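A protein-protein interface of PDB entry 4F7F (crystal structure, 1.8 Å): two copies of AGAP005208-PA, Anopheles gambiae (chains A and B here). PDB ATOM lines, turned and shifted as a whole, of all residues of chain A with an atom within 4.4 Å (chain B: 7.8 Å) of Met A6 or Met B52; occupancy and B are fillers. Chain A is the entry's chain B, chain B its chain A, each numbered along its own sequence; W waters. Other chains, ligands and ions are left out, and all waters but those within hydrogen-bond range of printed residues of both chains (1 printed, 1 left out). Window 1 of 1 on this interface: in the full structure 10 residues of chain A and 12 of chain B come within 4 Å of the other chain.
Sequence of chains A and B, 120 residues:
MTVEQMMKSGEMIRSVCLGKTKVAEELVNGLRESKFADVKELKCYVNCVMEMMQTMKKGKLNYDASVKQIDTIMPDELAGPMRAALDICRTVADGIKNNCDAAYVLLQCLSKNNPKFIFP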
ATOM      1  N   THR A   2     -19.358 -25.257 -21.513  1.00  0.00           N
ATOM      2  CA  THR A   2     -18.246 -25.209 -20.567  1.00  0.00           C
ATOM      3  C   THR A   2     -17.575 -23.821 -20.602  1.00  0.00           C
ATOM      4  O   THR A   2     -17.817 -23.017 -21.519  1.00  0.00           O
ATOM      5  CB  THR A   2     -17.214 -26.332 -20.853  1.00  0.00           C
ATOM      6  OG1 THR A   2     -16.574 -26.090 -22.115  1.00  0.00           O
ATOM      7  CG2 THR A   2     -17.907 -27.659 -20.924  1.00  0.00           C
ATOM      8  N   VAL A   3     -16.745 -23.527 -19.607  1.00  0.00           N
ATOM      9  CA  VAL A   3     -16.099 -22.221 -19.579  1.00  0.00           C
ATOM     10  C   VAL A   3     -15.099 -22.033 -20.723  1.00  0.00           C
ATOM     11  O   VAL A   3     -15.260 -21.124 -21.546  1.00  0.00           O
ATOM     12  CB  VAL A   3     -15.432 -21.903 -18.223  1.00  0.00           C
ATOM     13  CG1 VAL A   3     -14.650 -20.610 -18.330  1.00  0.00           C
ATOM     14  CG2 VAL A   3     -16.479 -21.786 -17.145  1.00  0.00           C
ATOM     15  N   GLU A   4     -14.071 -22.869 -20.802  1.00  0.00           N
ATOM     16  CA  GLU A   4     -13.010 -22.581 -21.771  1.00  0.00           C
ATOM     17  C   GLU A   4     -13.458 -22.643 -23.251  1.00  0.00           C
ATOM     18  O   GLU A   4     -12.828 -22.022 -24.112  1.00  0.00           O
ATOM     19  CB  GLU A   4     -11.743 -23.410 -21.501  1.00  0.00           C
ATOM     20  CG  GLU A   4     -10.424 -22.629 -21.711  1.00  0.00           C
ATOM     21  CD  GLU A   4      -9.274 -23.135 -20.825  1.00  0.00           C
ATOM     22  OE1 GLU A   4      -8.461 -22.305 -20.330  1.00  0.00           O
ATOM     23  OE2 GLU A   4      -9.186 -24.369 -20.618  1.00  0.00           O
ATOM     24  N   GLN A   5     -14.555 -23.346 -23.541  1.00  0.00           N
ATOM     25  CA  GLN A   5     -15.060 -23.420 -24.915  1.00  0.00           C
ATOM     26  C   GLN A   5     -15.973 -22.248 -25.224  1.00  0.00           C
ATOM     27  O   GLN A   5     -15.908 -21.684 -26.321  1.00  0.00           O
ATOM     28  CB  GLN A   5     -15.799 -24.746 -25.192  1.00  0.00           C
ATOM     29  CG  GLN A   5     -17.231 -24.815 -24.640  1.00  0.00           C
ATOM     30  CD  GLN A   5     -17.941 -26.120 -24.986  1.00  0.00           C
ATOM     31  OE1 GLN A   5     -18.458 -26.813 -24.104  1.00  0.00           O
ATOM     32  NE2 GLN A   5     -17.973 -26.458 -26.275  1.00  0.00           N
ATOM     33  N   MET A   6     -16.840 -21.889 -24.278  1.00  0.00           N
ATOM     34  CA  MET A   6     -17.569 -20.639 -24.412  1.00  0.00           C
ATOM     35  C   MET A   6     -16.565 -19.496 -24.625  1.00  0.00           C
ATOM     36  O   MET A   6     -16.759 -18.658 -25.497  1.00  0.00           O
ATOM     37  CB  MET A   6     -18.483 -20.345 -23.222  1.00  0.00           C
ATOM     38  CG  MET A   6     -19.281 -19.041 -23.406  1.00  0.00           C
ATOM     39  SD  MET A   6     -20.414 -18.563 -22.068  1.00  0.00           S
ATOM     40  CE  MET A   6     -19.260 -18.162 -20.746  1.00  0.00           C
ATOM     41  N   MET A   7     -15.486 -19.467 -23.849  1.00  0.00           N
ATOM     42  CA  MET A   7     -14.517 -18.377 -24.017  1.00  0.00           C
ATOM     43  C   MET A   7     -13.803 -18.403 -25.360  1.00  0.00           C
ATOM     44  O   MET A   7     -13.710 -17.377 -26.021  1.00  0.00           O
ATOM     45  CB  MET A   7     -13.494 -18.314 -22.881  1.00  0.00           C
ATOM     46  CG  MET A   7     -14.085 -18.078 -21.495  1.00  0.00           C
ATOM     47  SD  MET A   7     -15.172 -16.647 -21.396  1.00  0.00           S
ATOM     48  CE  MET A   7     -14.055 -15.293 -21.846  1.00  0.00           C
ATOM     49  N   LYS A   8     -13.306 -19.563 -25.777  1.00  0.00           N
ATOM     50  CA  LYS A   8     -12.582 -19.651 -27.047  1.00  0.00           C
ATOM     51  C   LYS A   8     -13.504 -19.330 -28.200  1.00  0.00           C
ATOM     52  O   LYS A   8     -13.134 -18.613 -29.126  1.00  0.00           O
ATOM     53  CB  LYS A   8     -12.002 -21.053 -27.254  1.00  0.00           C
ATOM     54  CG  LYS A   8     -11.032 -21.166 -28.433  1.00  0.00           C
ATOM     55  CD  LYS A   8     -10.419 -22.574 -28.518  1.00  0.00           C
ATOM     56  CE  LYS A   8      -9.384 -22.675 -29.641  1.00  0.00           C
ATOM     57  NZ  LYS A   8      -9.037 -24.093 -29.966  1.00  0.00           N
ATOM     58  N   SER A   9     -14.702 -19.899 -28.155  1.00  0.00           N
ATOM     59  CA  SER A   9     -15.677 -19.678 -29.207  1.00  0.00           C
ATOM     60  C   SER A   9     -16.132 -18.223 -29.255  1.00  0.00           C
ATOM     61  O   SER A   9     -16.126 -17.591 -30.333  1.00  0.00           O
ATOM     62  CB  SER A   9     -16.868 -20.626 -29.032  1.00  0.00           C
ATOM     63  OG  SER A   9     -17.126 -21.273 -30.262  1.00  0.00           O
ATOM     64  N   GLY A  10     -16.524 -17.694 -28.096  1.00  0.00           N
ATOM     65  CA  GLY A  10     -16.944 -16.311 -27.990  1.00  0.00           C
ATOM     66  C   GLY A  10     -15.862 -15.359 -28.493  1.00  0.00           C
ATOM     67  O   GLY A  10     -16.158 -14.403 -29.205  1.00  0.00           O
ATOM     68  N   ILE A  73     -22.937 -24.925 -25.505  1.00  0.00           N
ATOM     69  CA  ILE A  73     -21.889 -23.938 -25.277  1.00  0.00           C
ATOM     70  C   ILE A  73     -21.982 -23.259 -23.912  1.00  0.00           C
ATOM     71  O   ILE A  73     -20.961 -22.960 -23.302  1.00  0.00           O
ATOM     72  CB  ILE A  73     -21.877 -22.859 -26.389  1.00  0.00           C
ATOM     73  CG1 ILE A  73     -20.774 -21.836 -26.125  1.00  0.00           C
ATOM     74  CG2 ILE A  73     -23.231 -22.164 -26.500  1.00  0.00           C
ATOM     75  CD1 ILE A  73     -20.609 -20.825 -27.240  1.00  0.00           C
ATOM     76  N   PRO A  75     -22.596 -22.504 -19.884  1.00  0.00           N
ATOM     77  CA  PRO A  75     -22.652 -23.129 -18.557  1.00  0.00           C
ATOM     78  C   PRO A  75     -24.099 -23.233 -18.082  1.00  0.00           C
ATOM     79  O   PRO A  75     -24.845 -22.265 -18.201  1.00  0.00           O
ATOM     80  CB  PRO A  75     -21.884 -22.142 -17.680  1.00  0.00           C
ATOM     81  CG  PRO A  75     -20.928 -21.471 -18.627  1.00  0.00           C
ATOM     82  CD  PRO A  75     -21.662 -21.362 -19.928  1.00  0.00           C
ATOM     83  N   ILE A 118     -25.863 -12.672 -21.644  1.00  0.00           N
ATOM     84  CA  ILE A 118     -24.463 -12.523 -22.065  1.00  0.00           C
ATOM     85  C   ILE A 118     -24.329 -12.798 -23.567  1.00  0.00           C
ATOM     86  O   ILE A 118     -25.082 -13.599 -24.128  1.00  0.00           O
ATOM     87  CB  ILE A 118     -23.512 -13.468 -21.304  1.00  0.00           C
ATOM     88  CG1 ILE A 118     -22.061 -13.170 -21.701  1.00  0.00           C
ATOM     89  CG2 ILE A 118     -23.839 -14.921 -21.620  1.00  0.00           C
ATOM     90  CD1 ILE A 118     -21.065 -14.213 -21.218  1.00  0.00           C
ATOM     91  N   SER B   9     -21.150  -7.996 -13.725  1.00  0.00           N
ATOM     92  CA  SER B   9     -20.224  -9.015 -14.203  1.00  0.00           C
ATOM     93  C   SER B   9     -19.770  -9.929 -13.072  1.00  0.00           C
ATOM     94  O   SER B   9     -19.705 -11.143 -13.238  1.00  0.00           O
ATOM     95  CB  SER B   9     -19.007  -8.378 -14.866  1.00  0.00           C
ATOM     96  OG  SER B   9     -19.364  -7.729 -16.066  1.00  0.00           O
ATOM     97  N   MET B  12     -22.432 -12.345 -11.946  1.00  0.00           N
ATOM     98  CA  MET B  12     -22.680 -13.418 -12.867  1.00  0.00           C
ATOM     99  C   MET B  12     -21.531 -14.414 -12.817  1.00  0.00           C
ATOM    100  O   MET B  12     -21.765 -15.622 -12.796  1.00  0.00           O
ATOM    101  CB  MET B  12     -22.890 -12.898 -14.271  1.00  0.00           C
ATOM    102  CG  MET B  12     -23.130 -13.988 -15.292  1.00  0.00           C
ATOM    103  SD  MET B  12     -21.599 -14.326 -16.180  1.00  0.00           S
ATOM    104  CE  MET B  12     -21.874 -13.353 -17.666  1.00  0.00           C
ATOM    105  N   ILE B  13     -20.301 -13.908 -12.820  1.00  0.00           N
ATOM    106  CA  ILE B  13     -19.135 -14.792 -12.804  1.00  0.00           C
ATOM    107  C   ILE B  13     -19.100 -15.623 -11.529  1.00  0.00           C
ATOM    108  O   ILE B  13     -18.849 -16.843 -11.563  1.00  0.00           O
ATOM    109  CB  ILE B  13     -17.836 -14.004 -12.953  1.00  0.00           C
ATOM    110  CG1 ILE B  13     -17.689 -13.575 -14.398  1.00  0.00           C
ATOM    111  CG2 ILE B  13     -16.636 -14.848 -12.560  1.00  0.00           C
ATOM    112  CD1 ILE B  13     -16.662 -12.435 -14.590  1.00  0.00           C
ATOM    113  N   ARG B  14     -19.367 -14.982 -10.396  1.00  0.00           N
ATOM    114  CA  ARG B  14     -19.449 -15.755  -9.164  1.00  0.00           C
ATOM    115  C   ARG B  14     -20.434 -16.926  -9.293  1.00  0.00           C
ATOM    116  O   ARG B  14     -20.097 -18.061  -8.967  1.00  0.00           O
ATOM    117  CB  ARG B  14     -19.831 -14.923  -7.951  1.00  0.00           C
ATOM    118  CG  ARG B  14     -20.137 -15.859  -6.787  1.00  0.00           C
ATOM    119  CD  ARG B  14     -20.608 -15.166  -5.536  1.00  0.00           C
ATOM    120  NE  ARG B  14     -19.510 -14.476  -4.889  1.00  0.00           N
ATOM    121  CZ  ARG B  14     -19.351 -14.401  -3.575  1.00  0.00           C
ATOM    122  NH1 ARG B  14     -20.222 -14.990  -2.753  1.00  0.00           N
ATOM    123  NH2 ARG B  14     -18.330 -13.724  -3.090  1.00  0.00           N
ATOM    124  N   VAL B  16     -21.664 -18.558 -11.839  1.00  0.00           N
ATOM    125  CA  VAL B  16     -21.204 -19.579 -12.785  1.00  0.00           C
ATOM    126  C   VAL B  16     -20.074 -20.451 -12.206  1.00  0.00           C
ATOM    127  O   VAL B  16     -20.096 -21.700 -12.286  1.00  0.00           O
ATOM    128  CB  VAL B  16     -20.674 -18.931 -14.065  1.00  0.00           C
ATOM    129  CG1 VAL B  16     -19.926 -19.951 -14.910  1.00  0.00           C
ATOM    130  CG2 VAL B  16     -21.815 -18.296 -14.847  1.00  0.00           C
ATOM    131  N   CYS B  17     -19.076 -19.784 -11.644  1.00  0.00           N
ATOM    132  CA  CYS B  17     -17.888 -20.478 -11.152  1.00  0.00           C
ATOM    133  C   CYS B  17     -18.204 -21.222  -9.840  1.00  0.00           C
ATOM    134  O   CYS B  17     -17.624 -22.267  -9.590  1.00  0.00           O
ATOM    135  CB  CYS B  17     -16.722 -19.508 -11.019  1.00  0.00           C
ATOM    136  SG  CYS B  17     -16.141 -18.956 -12.678  1.00  0.00           S
ATOM    137  N   LYS B  20     -19.804 -24.389 -11.188  1.00  0.00           N
ATOM    138  CA  LYS B  20     -18.906 -25.287 -11.881  1.00  0.00           C
ATOM    139  C   LYS B  20     -17.934 -26.013 -10.947  1.00  0.00           C
ATOM    140  O   LYS B  20     -17.667 -27.204 -11.145  1.00  0.00           O
ATOM    141  CB  LYS B  20     -18.129 -24.575 -12.990  1.00  0.00           C
ATOM    142  CG  LYS B  20     -17.034 -25.456 -13.554  1.00  0.00           C
ATOM    143  CD  LYS B  20     -16.034 -24.691 -14.395  1.00  0.00           C
ATOM    144  CE  LYS B  20     -14.875 -25.609 -14.792  1.00  0.00           C
ATOM    145  NZ  LYS B  20     -14.519 -25.524 -16.244  1.00  0.00           N
ATOM    146  N   TYR B  45     -12.099 -22.527  -8.283  1.00  0.00           N
ATOM    147  CA  TYR B  45     -13.009 -21.388  -8.376  1.00  0.00           C
ATOM    148  C   TYR B  45     -12.233 -20.160  -8.896  1.00  0.00           C
ATOM    149  O   TYR B  45     -12.688 -19.452  -9.806  1.00  0.00           O
ATOM    150  CB  TYR B  45     -13.646 -21.043  -7.021  1.00  0.00           C
ATOM    151  CG  TYR B  45     -14.425 -19.738  -7.048  1.00  0.00           C
ATOM    152  CD1 TYR B  45     -15.726 -19.685  -7.551  1.00  0.00           C
ATOM    153  CD2 TYR B  45     -13.850 -18.549  -6.592  1.00  0.00           C
ATOM    154  CE1 TYR B  45     -16.430 -18.492  -7.562  1.00  0.00           C
ATOM    155  CE2 TYR B  45     -14.551 -17.361  -6.605  1.00  0.00           C
ATOM    156  CZ  TYR B  45     -15.830 -17.329  -7.112  1.00  0.00           C
ATOM    157  OH  TYR B  45     -16.508 -16.134  -7.143  1.00  0.00           O
ATOM    158  N   VAL B  46     -11.072 -19.907  -8.298  1.00  0.00           N
ATOM    159  CA  VAL B  46     -10.249 -18.753  -8.705  1.00  0.00           C
ATOM    160  C   VAL B  46      -9.845 -18.892 -10.168  1.00  0.00           C
ATOM    161  O   VAL B  46      -9.924 -17.920 -10.926  1.00  0.00           O
ATOM    162  CB  VAL B  46      -9.016 -18.616  -7.820  1.00  0.00           C
ATOM    163  CG1 VAL B  46      -7.997 -17.659  -8.444  1.00  0.00           C
ATOM    164  CG2 VAL B  46      -9.442 -18.177  -6.406  1.00  0.00           C
ATOM    165  N   ASN B  47      -9.421 -20.083 -10.582  1.00  0.00           N
ATOM    166  CA  ASN B  47      -9.083 -20.305 -11.981  1.00  0.00           C
ATOM    167  C   ASN B  47     -10.285 -20.021 -12.923  1.00  0.00           C
ATOM    168  O   ASN B  47     -10.154 -19.390 -13.971  1.00  0.00           O
ATOM    169  CB  ASN B  47      -8.561 -21.727 -12.196  1.00  0.00           C
ATOM    170  CG  ASN B  47      -8.156 -21.969 -13.626  1.00  0.00           C
ATOM    171  OD1 ASN B  47      -7.219 -21.329 -14.162  1.00  0.00           O
ATOM    172  ND2 ASN B  47      -8.860 -22.876 -14.271  1.00  0.00           N
ATOM    173  N   CYS B  48     -11.467 -20.481 -12.531  1.00  0.00           N
ATOM    174  CA  CYS B  48     -12.674 -20.220 -13.331  1.00  0.00           C
ATOM    175  C   CYS B  48     -12.948 -18.727 -13.492  1.00  0.00           C
ATOM    176  O   CYS B  48     -13.255 -18.241 -14.604  1.00  0.00           O
ATOM    177  CB  CYS B  48     -13.864 -20.882 -12.659  1.00  0.00           C
ATOM    178  SG  CYS B  48     -15.420 -20.707 -13.466  1.00  0.00           S
ATOM    179  N   VAL B  49     -12.841 -17.996 -12.388  1.00  0.00           N
ATOM    180  CA  VAL B  49     -13.002 -16.543 -12.461  1.00  0.00           C
ATOM    181  C   VAL B  49     -12.007 -15.893 -13.442  1.00  0.00           C
ATOM    182  O   VAL B  49     -12.396 -15.076 -14.288  1.00  0.00           O
ATOM    183  CB  VAL B  49     -12.858 -15.911 -11.089  1.00  0.00           C
ATOM    184  CG1 VAL B  49     -12.870 -14.424 -11.229  1.00  0.00           C
ATOM    185  CG2 VAL B  49     -14.012 -16.357 -10.186  1.00  0.00           C
ATOM    186  N   MET B  50     -10.726 -16.243 -13.325  1.00  0.00           N
ATOM    187  CA  MET B  50      -9.729 -15.679 -14.235  1.00  0.00           C
ATOM    188  C   MET B  50      -9.933 -16.080 -15.684  1.00  0.00           C
ATOM    189  O   MET B  50      -9.638 -15.299 -16.586  1.00  0.00           O
ATOM    190  CB  MET B  50      -8.320 -16.026 -13.760  1.00  0.00           C
ATOM    191  CG  MET B  50      -8.093 -15.522 -12.359  1.00  0.00           C
ATOM    192  SD  MET B  50      -6.389 -15.750 -11.930  1.00  0.00           S
ATOM    193  CE  MET B  50      -6.351 -14.594 -10.550  1.00  0.00           C
ATOM    194  N   GLU B  51     -10.432 -17.293 -15.931  1.00  0.00           N
ATOM    195  CA  GLU B  51     -10.750 -17.705 -17.297  1.00  0.00           C
ATOM    196  C   GLU B  51     -11.947 -16.927 -17.831  1.00  0.00           C
ATOM    197  O   GLU B  51     -11.927 -16.514 -18.984  1.00  0.00           O
ATOM    198  CB  GLU B  51     -11.025 -19.218 -17.411  1.00  0.00           C
ATOM    199  CG  GLU B  51      -9.756 -20.051 -17.339  1.00  0.00           C
ATOM    200  CD  GLU B  51     -10.025 -21.545 -17.251  1.00  0.00           C
ATOM    201  OE1 GLU B  51     -11.192 -21.952 -17.061  1.00  0.00           O
ATOM    202  OE2 GLU B  51      -9.054 -22.307 -17.394  1.00  0.00           O
ATOM    203  N   MET B  52     -12.974 -16.702 -17.011  1.00  0.00           N
ATOM    204  CA  MET B  52     -14.129 -15.905 -17.480  1.00  0.00           C
ATOM    205  C   MET B  52     -13.743 -14.442 -17.762  1.00  0.00           C
ATOM    206  O   MET B  52     -14.395 -13.730 -18.543  1.00  0.00           O
ATOM    207  CB  MET B  52     -15.292 -15.966 -16.470  1.00  0.00           C
ATOM    208  CG  MET B  52     -15.957 -17.327 -16.316  1.00  0.00           C
ATOM    209  SD  MET B  52     -17.289 -17.661 -17.481  1.00  0.00           S
ATOM    210  CE  MET B  52     -18.485 -16.381 -17.088  1.00  0.00           C
ATOM    211  N   MET B  53     -12.671 -13.998 -17.128  1.00  0.00           N
ATOM    212  CA  MET B  53     -12.169 -12.630 -17.302  1.00  0.00           C
ATOM    213  C   MET B  53     -11.045 -12.563 -18.328  1.00  0.00           C
ATOM    214  O   MET B  53     -10.418 -11.516 -18.480  1.00  0.00           O
ATOM    215  CB  MET B  53     -11.673 -12.078 -15.973  1.00  0.00           C
ATOM    216  CG  MET B  53     -12.767 -11.881 -14.962  1.00  0.00           C
ATOM    217  SD  MET B  53     -13.749 -10.417 -15.339  1.00  0.00           S
ATOM    218  CE  MET B  53     -12.554  -9.117 -15.020  1.00  0.00           C
ATOM    219  N   GLN B  54     -10.778 -13.679 -19.004  1.00  0.00           N
ATOM    220  CA  GLN B  54      -9.717 -13.733 -20.022  1.00  0.00           C
ATOM    221  C   GLN B  54      -8.308 -13.466 -19.489  1.00  0.00           C
ATOM    222  O   GLN B  54      -7.405 -13.153 -20.243  1.00  0.00           O
ATOM    223  CB  GLN B  54     -10.037 -12.786 -21.185  1.00  0.00           C
ATOM    224  CG  GLN B  54     -11.464 -12.974 -21.711  1.00  0.00           C
ATOM    225  CD  GLN B  54     -11.798 -12.164 -22.970  1.00  0.00           C
ATOM    226  OE1 GLN B  54     -12.855 -11.530 -23.057  1.00  0.00           O
ATOM    227  NE2 GLN B  54     -10.922 -12.221 -23.959  1.00  0.00           N
ATOM    228  N   THR B  55      -8.111 -13.640 -18.191  1.00  0.00           N
ATOM    229  CA  THR B  55      -6.838 -13.320 -17.580  1.00  0.00           C
ATOM    230  C   THR B  55      -5.902 -14.494 -17.605  1.00  0.00           C
ATOM    231  O   THR B  55      -4.676 -14.343 -17.644  1.00  0.00           O
ATOM    232  CB  THR B  55      -7.048 -12.869 -16.134  1.00  0.00           C
ATOM    233  OG1 THR B  55      -7.645 -11.573 -16.160  1.00  0.00           O
ATOM    234  CG2 THR B  55      -5.699 -12.783 -15.386  1.00  0.00           C
ATOM    235  N   MET B  56      -6.475 -15.682 -17.520  1.00  0.00           N
ATOM    236  CA  MET B  56      -5.701 -16.885 -17.703  1.00  0.00           C
ATOM    237  C   MET B  56      -6.359 -17.771 -18.727  1.00  0.00           C
ATOM    238  O   MET B  56      -7.584 -17.816 -18.831  1.00  0.00           O
ATOM    239  CB  MET B  56      -5.555 -17.632 -16.395  1.00  0.00           C
ATOM    240  CG  MET B  56      -4.542 -16.980 -15.484  1.00  0.00           C
ATOM    241  SD  MET B  56      -3.790 -18.319 -14.600  1.00  0.00           S
ATOM    242  CE  MET B  56      -2.195 -17.642 -14.172  1.00  0.00           C
ATOM    243  N   GLN B  69      -9.474  -6.229 -20.078  1.00  0.00           N
ATOM    244  CA  GLN B  69     -10.634  -6.554 -19.235  1.00  0.00           C
ATOM    245  C   GLN B  69     -10.710  -5.702 -17.986  1.00  0.00           C
ATOM    246  O   GLN B  69     -11.783  -5.182 -17.668  1.00  0.00           O
ATOM    247  CB  GLN B  69     -10.641  -8.032 -18.868  1.00  0.00           C
ATOM    248  CG  GLN B  69     -11.123  -8.910 -19.991  1.00  0.00           C
ATOM    249  CD  GLN B  69     -12.592  -8.697 -20.260  1.00  0.00           C
ATOM    250  OE1 GLN B  69     -12.969  -7.982 -21.184  1.00  0.00           O
ATOM    251  NE2 GLN B  69     -13.435  -9.307 -19.440  1.00  0.00           N
ATOM    252  N   ILE B  73     -13.948  -3.361 -17.267  1.00  0.00           N
ATOM    253  CA  ILE B  73     -14.908  -3.750 -16.239  1.00  0.00           C
ATOM    254  C   ILE B  73     -14.880  -2.832 -15.008  1.00  0.00           C
ATOM    255  O   ILE B  73     -15.938  -2.474 -14.469  1.00  0.00           O
ATOM    256  CB  ILE B  73     -14.668  -5.223 -15.796  1.00  0.00           C
ATOM    257  CG1 ILE B  73     -14.916  -6.180 -16.958  1.00  0.00           C
ATOM    258  CG2 ILE B  73     -15.603  -5.614 -14.665  1.00  0.00           C
ATOM    259  CD1 ILE B  73     -16.367  -6.607 -17.070  1.00  0.00           C
HETATM  260  O   HOH W   1     -11.788 -24.722 -18.312  1.00  0.00           O
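The side-chain carboxylate (OE1) of Glu A4 sits close to the side-chain carboxylate (OE2) of Glu B51, 3.0 Å away.
The side-chain sulfur (SG) of Cys B48 is disulfide-bonded to the side-chain sulfur (SG) of Cys B17, 2.1 Å away.
ND2 of Asn B47 lies within hydrogen-bond range of OE2 of Glu B51.
Val A3 touches Cys B48 (CG2 to SG, 3.98 Å).
Val A3 touches Glu B51 (CG1 to OE1, 3.9 Å).
CE of Met A6 touches SD of Met B52 (3.8 Å).
Met A7 touches Glu B51 (CG to O, 3.7 Å).
Met B52 touches Met A7 (O to CE, 3.7 Å).
CE of Met A7 touches CG of Gln B54, 3.5 Å away.
Met B12 touches Ile A118.
Of the printed residues of chain B, Val A3 touches Cys B48 and Glu B51.
Met A6 touches just one residue of chain B: Met B52 (3.8 Å).
Printed residues of chain B within 4 Å of Ile A118: Met B12.
Printed residues of chain A within 4 Å of Cys B48: Val A3.
Of the printed residues of chain A, Glu B51 touches Val A3 (3.9 Å), Glu A4 (3.0 Å) and Met A7 (3.7 Å).
Met B52 touches just these residues of chain A: Met A6 (3.8 Å) and Met A7 (3.7 Å).
Of the printed residues of chain A, Gln B54 touches Met A7.
The nearest residue of chain B that does not touch Met A6 is Val B16 (6.1 Å).
Of the 21 printed residues of chain B, 5 touch a printed residue of chain A.
Hydrophobic or aromatic side chains of chain B within 4 Å of the printed part of chain A: Met B12 and Met B52.
Of the 12 printed residues of chain A, 5 touch a printed residue of chain B.
2 positions are printed for both chains.
Water W1 bridges the side-chain carboxylate of Glu B51 (3.1 Å) and the side-chain carboxylate of Glu A4 (3.5 Å).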
